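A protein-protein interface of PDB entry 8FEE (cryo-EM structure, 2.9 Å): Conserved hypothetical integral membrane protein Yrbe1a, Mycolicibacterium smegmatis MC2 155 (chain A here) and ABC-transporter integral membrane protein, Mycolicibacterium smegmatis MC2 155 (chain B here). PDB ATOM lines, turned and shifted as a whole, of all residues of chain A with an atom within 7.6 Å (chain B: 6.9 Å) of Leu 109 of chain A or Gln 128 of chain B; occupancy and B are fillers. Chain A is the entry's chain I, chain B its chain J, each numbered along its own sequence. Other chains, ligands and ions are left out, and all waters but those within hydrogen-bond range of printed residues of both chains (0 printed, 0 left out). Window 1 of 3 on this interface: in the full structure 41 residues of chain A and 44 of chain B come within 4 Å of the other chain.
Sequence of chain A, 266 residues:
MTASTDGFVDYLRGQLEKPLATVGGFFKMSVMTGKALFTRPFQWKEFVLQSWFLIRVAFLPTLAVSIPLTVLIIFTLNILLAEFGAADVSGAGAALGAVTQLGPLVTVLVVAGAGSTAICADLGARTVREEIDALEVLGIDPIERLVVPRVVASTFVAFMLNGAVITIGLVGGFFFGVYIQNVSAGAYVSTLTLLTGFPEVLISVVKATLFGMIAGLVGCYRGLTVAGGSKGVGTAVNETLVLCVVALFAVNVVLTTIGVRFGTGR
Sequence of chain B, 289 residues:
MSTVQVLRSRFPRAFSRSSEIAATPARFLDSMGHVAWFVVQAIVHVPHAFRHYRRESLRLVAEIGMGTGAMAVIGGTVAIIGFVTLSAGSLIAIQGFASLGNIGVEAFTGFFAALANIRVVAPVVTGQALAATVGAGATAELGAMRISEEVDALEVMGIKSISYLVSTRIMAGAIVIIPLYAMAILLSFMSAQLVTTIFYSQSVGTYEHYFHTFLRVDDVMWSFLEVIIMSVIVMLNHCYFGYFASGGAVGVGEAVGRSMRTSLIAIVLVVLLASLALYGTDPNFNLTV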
ATOM      1  N   VAL A  65       5.429   5.615  -9.809  1.00  0.00           N
ATOM      2  CA  VAL A  65       5.326   6.024  -8.412  1.00  0.00           C
ATOM      3  C   VAL A  65       6.720   6.304  -7.859  1.00  0.00           C
ATOM      4  O   VAL A  65       6.901   7.207  -7.036  1.00  0.00           O
ATOM      5  CB  VAL A  65       4.586   4.964  -7.574  1.00  0.00           C
ATOM      6  CG1 VAL A  65       4.604   5.320  -6.099  1.00  0.00           C
ATOM      7  CG2 VAL A  65       3.147   4.842  -8.040  1.00  0.00           C
ATOM      8  N   LEU A  69       8.442  10.238  -6.599  1.00  0.00           N
ATOM      9  CA  LEU A  69       8.704  10.183  -5.163  1.00  0.00           C
ATOM     10  C   LEU A  69      10.178  10.423  -4.860  1.00  0.00           C
ATOM     11  O   LEU A  69      10.521  11.203  -3.960  1.00  0.00           O
ATOM     12  CB  LEU A  69       8.252   8.837  -4.598  1.00  0.00           C
ATOM     13  CG  LEU A  69       8.189   8.728  -3.076  1.00  0.00           C
ATOM     14  CD1 LEU A  69       7.289   9.805  -2.499  1.00  0.00           C
ATOM     15  CD2 LEU A  69       7.710   7.348  -2.663  1.00  0.00           C
ATOM     16  N   LEU A 102      12.845   3.886   0.672  1.00  0.00           N
ATOM     17  CA  LEU A 102      12.120   4.183  -0.562  1.00  0.00           C
ATOM     18  C   LEU A 102      11.878   2.927  -1.388  1.00  0.00           C
ATOM     19  O   LEU A 102      10.769   2.711  -1.887  1.00  0.00           O
ATOM     20  CB  LEU A 102      12.886   5.228  -1.377  1.00  0.00           C
ATOM     21  CG  LEU A 102      12.235   5.824  -2.628  1.00  0.00           C
ATOM     22  CD1 LEU A 102      12.626   7.278  -2.759  1.00  0.00           C
ATOM     23  CD2 LEU A 102      12.642   5.073  -3.887  1.00  0.00           C
ATOM     24  N   GLY A 103      12.894   2.082  -1.527  1.00  0.00           N
ATOM     25  CA  GLY A 103      12.767   0.842  -2.255  1.00  0.00           C
ATOM     26  C   GLY A 103      11.708  -0.085  -1.688  1.00  0.00           C
ATOM     27  O   GLY A 103      10.731  -0.433  -2.362  1.00  0.00           O
ATOM     28  N   PRO A 104      11.898  -0.520  -0.437  1.00  0.00           N
ATOM     29  CA  PRO A 104      10.886  -1.385   0.194  1.00  0.00           C
ATOM     30  C   PRO A 104       9.499  -0.773   0.289  1.00  0.00           C
ATOM     31  O   PRO A 104       8.514  -1.496   0.117  1.00  0.00           O
ATOM     32  CB  PRO A 104      11.487  -1.651   1.580  1.00  0.00           C
ATOM     33  CG  PRO A 104      12.947  -1.579   1.357  1.00  0.00           C
ATOM     34  CD  PRO A 104      13.145  -0.484   0.349  1.00  0.00           C
ATOM     35  N   LEU A 105       9.375   0.531   0.542  1.00  0.00           N
ATOM     36  CA  LEU A 105       8.039   1.107   0.687  1.00  0.00           C
ATOM     37  C   LEU A 105       7.333   1.258  -0.655  1.00  0.00           C
ATOM     38  O   LEU A 105       6.121   1.027  -0.751  1.00  0.00           O
ATOM     39  CB  LEU A 105       8.109   2.450   1.410  1.00  0.00           C
ATOM     40  CG  LEU A 105       8.085   2.332   2.933  1.00  0.00           C
ATOM     41  CD1 LEU A 105       8.057   3.703   3.568  1.00  0.00           C
ATOM     42  CD2 LEU A 105       6.883   1.514   3.371  1.00  0.00           C
ATOM     43  N   VAL A 106       8.059   1.666  -1.699  1.00  0.00           N
ATOM     44  CA  VAL A 106       7.469   1.680  -3.035  1.00  0.00           C
ATOM     45  C   VAL A 106       7.075   0.269  -3.451  1.00  0.00           C
ATOM     46  O   VAL A 106       6.015   0.058  -4.057  1.00  0.00           O
ATOM     47  CB  VAL A 106       8.436   2.333  -4.042  1.00  0.00           C
ATOM     48  CG1 VAL A 106       8.023   2.024  -5.469  1.00  0.00           C
ATOM     49  CG2 VAL A 106       8.471   3.834  -3.829  1.00  0.00           C
ATOM     50  N   THR A 107       7.904  -0.723  -3.108  1.00  0.00           N
ATOM     51  CA  THR A 107       7.536  -2.109  -3.374  1.00  0.00           C
ATOM     52  C   THR A 107       6.266  -2.495  -2.625  1.00  0.00           C
ATOM     53  O   THR A 107       5.369  -3.116  -3.200  1.00  0.00           O
ATOM     54  CB  THR A 107       8.693  -3.037  -2.999  1.00  0.00           C
ATOM     55  OG1 THR A 107       9.737  -2.917  -3.974  1.00  0.00           O
ATOM     56  CG2 THR A 107       8.233  -4.486  -2.937  1.00  0.00           C
ATOM     57  N   VAL A 108       6.156  -2.092  -1.355  1.00  0.00           N
ATOM     58  CA  VAL A 108       4.962  -2.383  -0.563  1.00  0.00           C
ATOM     59  C   VAL A 108       3.726  -1.804  -1.234  1.00  0.00           C
ATOM     60  O   VAL A 108       2.733  -2.506  -1.465  1.00  0.00           O
ATOM     61  CB  VAL A 108       5.118  -1.836   0.868  1.00  0.00           C
ATOM     62  CG1 VAL A 108       3.758  -1.682   1.534  1.00  0.00           C
ATOM     63  CG2 VAL A 108       5.991  -2.741   1.691  1.00  0.00           C
ATOM     64  N   LEU A 109       3.784  -0.516  -1.577  1.00  0.00           N
ATOM     65  CA  LEU A 109       2.626   0.147  -2.167  1.00  0.00           C
ATOM     66  C   LEU A 109       2.231  -0.499  -3.487  1.00  0.00           C
ATOM     67  O   LEU A 109       1.082  -0.916  -3.661  1.00  0.00           O
ATOM     68  CB  LEU A 109       2.918   1.635  -2.364  1.00  0.00           C
ATOM     69  CG  LEU A 109       3.115   2.471  -1.100  1.00  0.00           C
ATOM     70  CD1 LEU A 109       3.398   3.921  -1.459  1.00  0.00           C
ATOM     71  CD2 LEU A 109       1.900   2.366  -0.196  1.00  0.00           C
ATOM     72  N   VAL A 110       3.178  -0.624  -4.419  1.00  0.00           N
ATOM     73  CA  VAL A 110       2.810  -1.087  -5.753  1.00  0.00           C
ATOM     74  C   VAL A 110       2.547  -2.587  -5.805  1.00  0.00           C
ATOM     75  O   VAL A 110       1.689  -3.018  -6.585  1.00  0.00           O
ATOM     76  CB  VAL A 110       3.899  -0.687  -6.763  1.00  0.00           C
ATOM     77  CG1 VAL A 110       3.468  -1.013  -8.184  1.00  0.00           C
ATOM     78  CG2 VAL A 110       4.208   0.795  -6.640  1.00  0.00           C
ATOM     79  N   VAL A 111       3.013  -3.349  -4.817  1.00  0.00           N
ATOM     80  CA  VAL A 111       2.695  -4.771  -4.774  1.00  0.00           C
ATOM     81  C   VAL A 111       1.335  -4.989  -4.144  1.00  0.00           C
ATOM     82  O   VAL A 111       0.486  -5.661  -4.738  1.00  0.00           O
ATOM     83  CB  VAL A 111       3.802  -5.553  -4.042  1.00  0.00           C
ATOM     84  CG1 VAL A 111       3.288  -6.910  -3.608  1.00  0.00           C
ATOM     85  CG2 VAL A 111       5.003  -5.732  -4.956  1.00  0.00           C
ATOM     86  N   ALA A 112       1.091  -4.405  -2.967  1.00  0.00           N
ATOM     87  CA  ALA A 112      -0.216  -4.559  -2.343  1.00  0.00           C
ATOM     88  C   ALA A 112      -1.304  -4.013  -3.256  1.00  0.00           C
ATOM     89  O   ALA A 112      -2.372  -4.622  -3.389  1.00  0.00           O
ATOM     90  CB  ALA A 112      -0.238  -3.855  -0.987  1.00  0.00           C
ATOM     91  N   GLY A 113      -1.060  -2.863  -3.890  1.00  0.00           N
ATOM     92  CA  GLY A 113      -2.065  -2.296  -4.770  1.00  0.00           C
ATOM     93  C   GLY A 113      -2.300  -3.114  -6.026  1.00  0.00           C
ATOM     94  O   GLY A 113      -3.450  -3.317  -6.427  1.00  0.00           O
ATOM     95  N   ALA A 114      -1.233  -3.600  -6.671  1.00  0.00           N
ATOM     96  CA  ALA A 114      -1.394  -4.238  -7.971  1.00  0.00           C
ATOM     97  C   ALA A 114      -1.405  -5.762  -7.891  1.00  0.00           C
ATOM     98  O   ALA A 114      -2.416  -6.394  -8.204  1.00  0.00           O
ATOM     99  CB  ALA A 114      -0.287  -3.764  -8.920  1.00  0.00           C
ATOM    100  N   GLY A 115      -0.307  -6.360  -7.423  1.00  0.00           N
ATOM    101  CA  GLY A 115      -0.166  -7.804  -7.522  1.00  0.00           C
ATOM    102  C   GLY A 115      -1.018  -8.573  -6.533  1.00  0.00           C
ATOM    103  O   GLY A 115      -1.634  -9.582  -6.889  1.00  0.00           O
ATOM    104  N   PHE A 211       8.161  -9.121   1.973  1.00  0.00           N
ATOM    105  CA  PHE A 211       6.963  -8.423   1.519  1.00  0.00           C
ATOM    106  C   PHE A 211       6.282  -9.186   0.395  1.00  0.00           C
ATOM    107  O   PHE A 211       5.057  -9.345   0.396  1.00  0.00           O
ATOM    108  CB  PHE A 211       7.318  -7.009   1.058  1.00  0.00           C
ATOM    109  CG  PHE A 211       7.800  -6.112   2.158  1.00  0.00           C
ATOM    110  CD1 PHE A 211       7.483  -6.375   3.478  1.00  0.00           C
ATOM    111  CD2 PHE A 211       8.589  -5.012   1.869  1.00  0.00           C
ATOM    112  CE1 PHE A 211       7.933  -5.554   4.486  1.00  0.00           C
ATOM    113  CE2 PHE A 211       9.041  -4.189   2.872  1.00  0.00           C
ATOM    114  CZ  PHE A 211       8.714  -4.461   4.180  1.00  0.00           C
ATOM    115  N   LEU A 241      -6.185  -5.787   0.076  1.00  0.00           N
ATOM    116  CA  LEU A 241      -5.316  -4.621  -0.001  1.00  0.00           C
ATOM    117  C   LEU A 241      -5.056  -4.026   1.376  1.00  0.00           C
ATOM    118  O   LEU A 241      -3.913  -3.691   1.708  1.00  0.00           O
ATOM    119  CB  LEU A 241      -5.940  -3.586  -0.928  1.00  0.00           C
ATOM    120  CG  LEU A 241      -5.309  -2.204  -0.935  1.00  0.00           C
ATOM    121  CD1 LEU A 241      -3.936  -2.243  -1.573  1.00  0.00           C
ATOM    122  CD2 LEU A 241      -6.231  -1.284  -1.681  1.00  0.00           C
ATOM    123  N   VAL A 245      -1.408  -3.920   3.211  1.00  0.00           N
ATOM    124  CA  VAL A 245      -0.798  -2.648   3.594  1.00  0.00           C
ATOM    125  C   VAL A 245      -0.388  -2.676   5.061  1.00  0.00           C
ATOM    126  O   VAL A 245       0.762  -2.370   5.409  1.00  0.00           O
ATOM    127  CB  VAL A 245      -1.756  -1.481   3.291  1.00  0.00           C
ATOM    128  CG1 VAL A 245      -1.364  -0.246   4.085  1.00  0.00           C
ATOM    129  CG2 VAL A 245      -1.759  -1.175   1.803  1.00  0.00           C
ATOM    130  N   LEU A 248       2.467  -5.355   5.800  1.00  0.00           N
ATOM    131  CA  LEU A 248       3.757  -4.963   5.248  1.00  0.00           C
ATOM    132  C   LEU A 248       4.344  -3.771   5.990  1.00  0.00           C
ATOM    133  O   LEU A 248       5.561  -3.705   6.179  1.00  0.00           O
ATOM    134  CB  LEU A 248       3.635  -4.670   3.754  1.00  0.00           C
ATOM    135  CG  LEU A 248       3.287  -5.859   2.852  1.00  0.00           C
ATOM    136  CD1 LEU A 248       3.584  -5.549   1.393  1.00  0.00           C
ATOM    137  CD2 LEU A 248       4.000  -7.122   3.301  1.00  0.00           C
ATOM    138  N   PHE A 249       3.510  -2.823   6.430  1.00  0.00           N
ATOM    139  CA  PHE A 249       4.055  -1.709   7.202  1.00  0.00           C
ATOM    140  C   PHE A 249       4.602  -2.174   8.550  1.00  0.00           C
ATOM    141  O   PHE A 249       5.679  -1.730   8.973  1.00  0.00           O
ATOM    142  CB  PHE A 249       3.001  -0.616   7.385  1.00  0.00           C
ATOM    143  CG  PHE A 249       3.038   0.438   6.313  1.00  0.00           C
ATOM    144  CD1 PHE A 249       2.317   0.288   5.142  1.00  0.00           C
ATOM    145  CD2 PHE A 249       3.806   1.578   6.475  1.00  0.00           C
ATOM    146  CE1 PHE A 249       2.358   1.255   4.157  1.00  0.00           C
ATOM    147  CE2 PHE A 249       3.851   2.547   5.495  1.00  0.00           C
ATOM    148  CZ  PHE A 249       3.125   2.385   4.334  1.00  0.00           C
ATOM    149  N   ILE B  81      -5.674   4.403   9.002  1.00  0.00           N
ATOM    150  CA  ILE B  81      -4.878   5.619   8.854  1.00  0.00           C
ATOM    151  C   ILE B  81      -3.945   5.779  10.044  1.00  0.00           C
ATOM    152  O   ILE B  81      -2.749   6.066   9.889  1.00  0.00           O
ATOM    153  CB  ILE B  81      -5.802   6.842   8.697  1.00  0.00           C
ATOM    154  CG1 ILE B  81      -6.407   6.897   7.292  1.00  0.00           C
ATOM    155  CG2 ILE B  81      -5.058   8.132   9.019  1.00  0.00           C
ATOM    156  CD1 ILE B  81      -5.471   7.442   6.243  1.00  0.00           C
ATOM    157  N   VAL B  84      -1.010   3.115   9.923  1.00  0.00           N
ATOM    158  CA  VAL B  84      -0.014   3.342   8.880  1.00  0.00           C
ATOM    159  C   VAL B  84       0.809   4.591   9.183  1.00  0.00           C
ATOM    160  O   VAL B  84       2.030   4.614   8.976  1.00  0.00           O
ATOM    161  CB  VAL B  84      -0.685   3.410   7.497  1.00  0.00           C
ATOM    162  CG1 VAL B  84       0.356   3.577   6.419  1.00  0.00           C
ATOM    163  CG2 VAL B  84      -1.468   2.140   7.236  1.00  0.00           C
ATOM    164  N   ALA B 122       4.158  12.137   5.615  1.00  0.00           N
ATOM    165  CA  ALA B 122       2.784  12.087   6.117  1.00  0.00           C
ATOM    166  C   ALA B 122       1.734  12.350   5.044  1.00  0.00           C
ATOM    167  O   ALA B 122       0.760  11.580   4.978  1.00  0.00           O
ATOM    168  CB  ALA B 122       2.628  13.036   7.311  1.00  0.00           C
ATOM    169  N   PRO B 123       1.844  13.380   4.186  1.00  0.00           N
ATOM    170  CA  PRO B 123       0.834  13.527   3.120  1.00  0.00           C
ATOM    171  C   PRO B 123       0.737  12.316   2.210  1.00  0.00           C
ATOM    172  O   PRO B 123      -0.369  11.827   1.960  1.00  0.00           O
ATOM    173  CB  PRO B 123       1.308  14.774   2.364  1.00  0.00           C
ATOM    174  CG  PRO B 123       2.045  15.551   3.362  1.00  0.00           C
ATOM    175  CD  PRO B 123       2.758  14.540   4.200  1.00  0.00           C
ATOM    176  N   VAL B 124       1.870  11.812   1.717  1.00  0.00           N
ATOM    177  CA  VAL B 124       1.847  10.705   0.765  1.00  0.00           C
ATOM    178  C   VAL B 124       1.286   9.446   1.416  1.00  0.00           C
ATOM    179  O   VAL B 124       0.441   8.754   0.839  1.00  0.00           O
ATOM    180  CB  VAL B 124       3.254  10.462   0.191  1.00  0.00           C
ATOM    181  CG1 VAL B 124       3.269   9.219  -0.678  1.00  0.00           C
ATOM    182  CG2 VAL B 124       3.715  11.669  -0.601  1.00  0.00           C
ATOM    183  N   VAL B 125       1.740   9.135   2.631  1.00  0.00           N
ATOM    184  CA  VAL B 125       1.309   7.914   3.306  1.00  0.00           C
ATOM    185  C   VAL B 125      -0.167   7.989   3.682  1.00  0.00           C
ATOM    186  O   VAL B 125      -0.919   7.021   3.493  1.00  0.00           O
ATOM    187  CB  VAL B 125       2.208   7.656   4.528  1.00  0.00           C
ATOM    188  CG1 VAL B 125       1.471   6.882   5.599  1.00  0.00           C
ATOM    189  CG2 VAL B 125       3.463   6.911   4.107  1.00  0.00           C
ATOM    190  N   THR B 126      -0.611   9.134   4.214  1.00  0.00           N
ATOM    191  CA  THR B 126      -2.029   9.312   4.507  1.00  0.00           C
ATOM    192  C   THR B 126      -2.859   9.210   3.237  1.00  0.00           C
ATOM    193  O   THR B 126      -3.946   8.622   3.243  1.00  0.00           O
ATOM    194  CB  THR B 126      -2.255  10.658   5.192  1.00  0.00           C
ATOM    195  OG1 THR B 126      -1.470  10.722   6.388  1.00  0.00           O
ATOM    196  CG2 THR B 126      -3.722  10.841   5.550  1.00  0.00           C
ATOM    197  N   GLY B 127      -2.349   9.754   2.131  1.00  0.00           N
ATOM    198  CA  GLY B 127      -3.057   9.647   0.871  1.00  0.00           C
ATOM    199  C   GLY B 127      -3.191   8.218   0.391  1.00  0.00           C
ATOM    200  O   GLY B 127      -4.256   7.815  -0.069  1.00  0.00           O
ATOM    201  N   GLN B 128      -2.114   7.435   0.485  1.00  0.00           N
ATOM    202  CA  GLN B 128      -2.181   6.047   0.031  1.00  0.00           C
ATOM    203  C   GLN B 128      -3.119   5.219   0.902  1.00  0.00           C
ATOM    204  O   GLN B 128      -3.893   4.403   0.387  1.00  0.00           O
ATOM    205  CB  GLN B 128      -0.788   5.416   0.000  1.00  0.00           C
ATOM    206  CG  GLN B 128       0.268   6.158  -0.824  1.00  0.00           C
ATOM    207  CD  GLN B 128       0.075   6.066  -2.333  1.00  0.00           C
ATOM    208  OE1 GLN B 128      -1.046   6.025  -2.838  1.00  0.00           O
ATOM    209  NE2 GLN B 128       1.185   6.038  -3.060  1.00  0.00           N
ATOM    210  N   ALA B 129      -3.064   5.410   2.222  1.00  0.00           N
ATOM    211  CA  ALA B 129      -3.971   4.677   3.103  1.00  0.00           C
ATOM    212  C   ALA B 129      -5.425   5.078   2.870  1.00  0.00           C
ATOM    213  O   ALA B 129      -6.317   4.217   2.846  1.00  0.00           O
ATOM    214  CB  ALA B 129      -3.573   4.895   4.561  1.00  0.00           C
ATOM    215  N   LEU B 130      -5.684   6.380   2.698  1.00  0.00           N
ATOM    216  CA  LEU B 130      -7.033   6.839   2.387  1.00  0.00           C
ATOM    217  C   LEU B 130      -7.503   6.292   1.050  1.00  0.00           C
ATOM    218  O   LEU B 130      -8.651   5.853   0.923  1.00  0.00           O
ATOM    219  CB  LEU B 130      -7.073   8.367   2.370  1.00  0.00           C
ATOM    220  CG  LEU B 130      -8.389   8.993   1.908  1.00  0.00           C
ATOM    221  CD1 LEU B 130      -9.380   9.083   3.055  1.00  0.00           C
ATOM    222  CD2 LEU B 130      -8.153  10.351   1.273  1.00  0.00           C
ATOM    223  N   ALA B 131      -6.622   6.312   0.044  1.00  0.00           N
ATOM    224  CA  ALA B 131      -6.913   5.713  -1.249  1.00  0.00           C
ATOM    225  C   ALA B 131      -7.376   4.281  -1.070  1.00  0.00           C
ATOM    226  O   ALA B 131      -8.520   3.955  -1.392  1.00  0.00           O
ATOM    227  CB  ALA B 131      -5.679   5.777  -2.151  1.00  0.00           C
ATOM    228  N   ALA B 132      -6.528   3.447  -0.461  1.00  0.00           N
ATOM    229  CA  ALA B 132      -6.850   2.048  -0.212  1.00  0.00           C
ATOM    230  C   ALA B 132      -8.226   1.926   0.423  1.00  0.00           C
ATOM    231  O   ALA B 132      -9.182   1.540  -0.258  1.00  0.00           O
ATOM    232  CB  ALA B 132      -5.793   1.407   0.689  1.00  0.00           C
ATOM    233  N   THR B 133      -8.368   2.413   1.656  1.00  0.00           N
ATOM    234  CA  THR B 133      -9.598   2.196   2.409  1.00  0.00           C
ATOM    235  C   THR B 133     -10.817   2.793   1.715  1.00  0.00           C
ATOM    236  O   THR B 133     -11.663   2.058   1.183  1.00  0.00           O
ATOM    237  CB  THR B 133      -9.466   2.782   3.815  1.00  0.00           C
ATOM    238  OG1 THR B 133      -9.031   4.142   3.723  1.00  0.00           O
ATOM    239  CG2 THR B 133      -8.463   1.988   4.629  1.00  0.00           C
ATOM    240  N   MET B 230      -5.650  16.302  -3.161  1.00  0.00           N
ATOM    241  CA  MET B 230      -5.348  14.908  -3.461  1.00  0.00           C
ATOM    242  C   MET B 230      -6.543  14.011  -3.170  1.00  0.00           C
ATOM    243  O   MET B 230      -6.849  13.108  -3.951  1.00  0.00           O
ATOM    244  CB  MET B 230      -4.129  14.467  -2.650  1.00  0.00           C
ATOM    245  CG  MET B 230      -4.177  13.038  -2.151  1.00  0.00           C
ATOM    246  SD  MET B 230      -3.401  12.881  -0.535  1.00  0.00           S
ATOM    247  CE  MET B 230      -1.836  13.686  -0.832  1.00  0.00           C
ATOM    248  N   MET B 260      -6.752   1.553  -7.699  1.00  0.00           N
ATOM    249  CA  MET B 260      -5.668   1.709  -6.734  1.00  0.00           C
ATOM    250  C   MET B 260      -4.372   2.133  -7.408  1.00  0.00           C
ATOM    251  O   MET B 260      -3.659   3.003  -6.892  1.00  0.00           O
ATOM    252  CB  MET B 260      -5.470   0.412  -5.959  1.00  0.00           C
ATOM    253  CG  MET B 260      -6.454   0.260  -4.836  1.00  0.00           C
ATOM    254  SD  MET B 260      -6.441   1.712  -3.771  1.00  0.00           S
ATOM    255  CE  MET B 260      -4.731   1.737  -3.234  1.00  0.00           C
ATOM    256  N   SER B 263      -4.688   5.730  -8.289  1.00  0.00           N
ATOM    257  CA  SER B 263      -4.645   6.559  -7.091  1.00  0.00           C
ATOM    258  C   SER B 263      -3.216   6.745  -6.600  1.00  0.00           C
ATOM    259  O   SER B 263      -2.831   7.853  -6.211  1.00  0.00           O
ATOM    260  CB  SER B 263      -5.509   5.940  -5.996  1.00  0.00           C
ATOM    261  OG  SER B 263      -6.852   5.831  -6.424  1.00  0.00           O
ATOM    262  N   LEU B 264      -2.422   5.667  -6.593  1.00  0.00           N
ATOM    263  CA  LEU B 264      -1.015   5.785  -6.212  1.00  0.00           C
ATOM    264  C   LEU B 264      -0.319   6.833  -7.070  1.00  0.00           C
ATOM    265  O   LEU B 264       0.319   7.768  -6.553  1.00  0.00           O
ATOM    266  CB  LEU B 264      -0.296   4.439  -6.356  1.00  0.00           C
ATOM    267  CG  LEU B 264      -0.770   3.152  -5.678  1.00  0.00           C
ATOM    268  CD1 LEU B 264      -0.047   1.959  -6.282  1.00  0.00           C
ATOM    269  CD2 LEU B 264      -0.553   3.187  -4.182  1.00  0.00           C
ATOM    270  N   ILE B 265      -0.452   6.692  -8.394  1.00  0.00           N
ATOM    271  CA  ILE B 265       0.250   7.594  -9.308  1.00  0.00           C
ATOM    272  C   ILE B 265      -0.203   9.034  -9.089  1.00  0.00           C
ATOM    273  O   ILE B 265       0.618   9.960  -9.009  1.00  0.00           O
ATOM    274  CB  ILE B 265       0.037   7.150 -10.766  1.00  0.00           C
ATOM    275  CG1 ILE B 265       0.564   5.730 -10.971  1.00  0.00           C
ATOM    276  CG2 ILE B 265       0.723   8.112 -11.718  1.00  0.00           C
ATOM    277  CD1 ILE B 265       0.459   5.241 -12.398  1.00  0.00           C
ATOM    278  N   ILE B 267      -1.625  10.504  -6.431  1.00  0.00           N
ATOM    279  CA  ILE B 267      -1.220  11.073  -5.146  1.00  0.00           C
ATOM    280  C   ILE B 267       0.241  11.495  -5.187  1.00  0.00           C
ATOM    281  O   ILE B 267       0.602  12.602  -4.756  1.00  0.00           O
ATOM    282  CB  ILE B 267      -1.475  10.067  -4.011  1.00  0.00           C
ATOM    283  CG1 ILE B 267      -2.971   9.864  -3.813  1.00  0.00           C
ATOM    284  CG2 ILE B 267      -0.832  10.540  -2.718  1.00  0.00           C
ATOM    285  CD1 ILE B 267      -3.304   8.649  -3.008  1.00  0.00           C
ATOM    286  N   VAL B 268       1.104  10.618  -5.709  1.00  0.00           N
ATOM    287  CA  VAL B 268       2.527  10.947  -5.740  1.00  0.00           C
ATOM    288  C   VAL B 268       2.772  12.168  -6.623  1.00  0.00           C
ATOM    289  O   VAL B 268       3.525  13.080  -6.250  1.00  0.00           O
ATOM    290  CB  VAL B 268       3.350   9.728  -6.189  1.00  0.00           C
ATOM    291  CG1 VAL B 268       4.807  10.099  -6.301  1.00  0.00           C
ATOM    292  CG2 VAL B 268       3.177   8.595  -5.198  1.00  0.00           C
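Of chain B, only Gln 128 comes within 4 Å of Leu 109 of chain A.
Of the printed residues of chain B, Phe 249 of chain A touches Val 84.
Of the printed residues of chain B, Val 65 of chain A touches Leu 264 (3.9 Å) and Val 268 (3.6 Å).
Printed residues of chain A within 4 Å of Ala 132 of chain B: Leu 241.
Thr 107 of chain A touches none of the printed residues of chain B.
Ile 265 of chain B touches none of the printed residues of chain A.
Leu 264 of chain B touches Val 65 of chain A (CB to CG2, 3.9 Å).
Val 268 of chain B touches Val 65 of chain A (CG1 to O, 3.6 Å).
Leu 69 of chain A touches Val 268 of chain B.
Leu 109 of chain A touches Gln 128 of chain B.
Leu 241 of chain A touches Ala 132 of chain B.
Leu 241 of chain A touches Met 260 of chain B (CD2 to CG, 3.5 Å).
CG1 of Val 245 of chain A touches CG2 of Val 84 of chain B (3.95 Å).
Phe 249 of chain A touches Val 84 of chain B (CZ to CG1, 3.7 Å).
The side-chain sulfur of Met 260 of chain B sits close to the backbone NH of Ala 132 of chain B (3.7 Å).
Hydrophobic or aromatic side chains of chain A that line the printed part of chain B: Val 65, Leu 109, Leu 241, Val 245 and Phe 249.
Of the 21 printed residues of chain B, 6 touch a printed residue of chain A.
Hydrophobic or aromatic side chains of chain B within 4 Å of the printed part of chain A: Val 84, Ala 132, Met 260, Leu 264 and Val 268.
Among the printed residues, 8 pairs touch across the chains.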
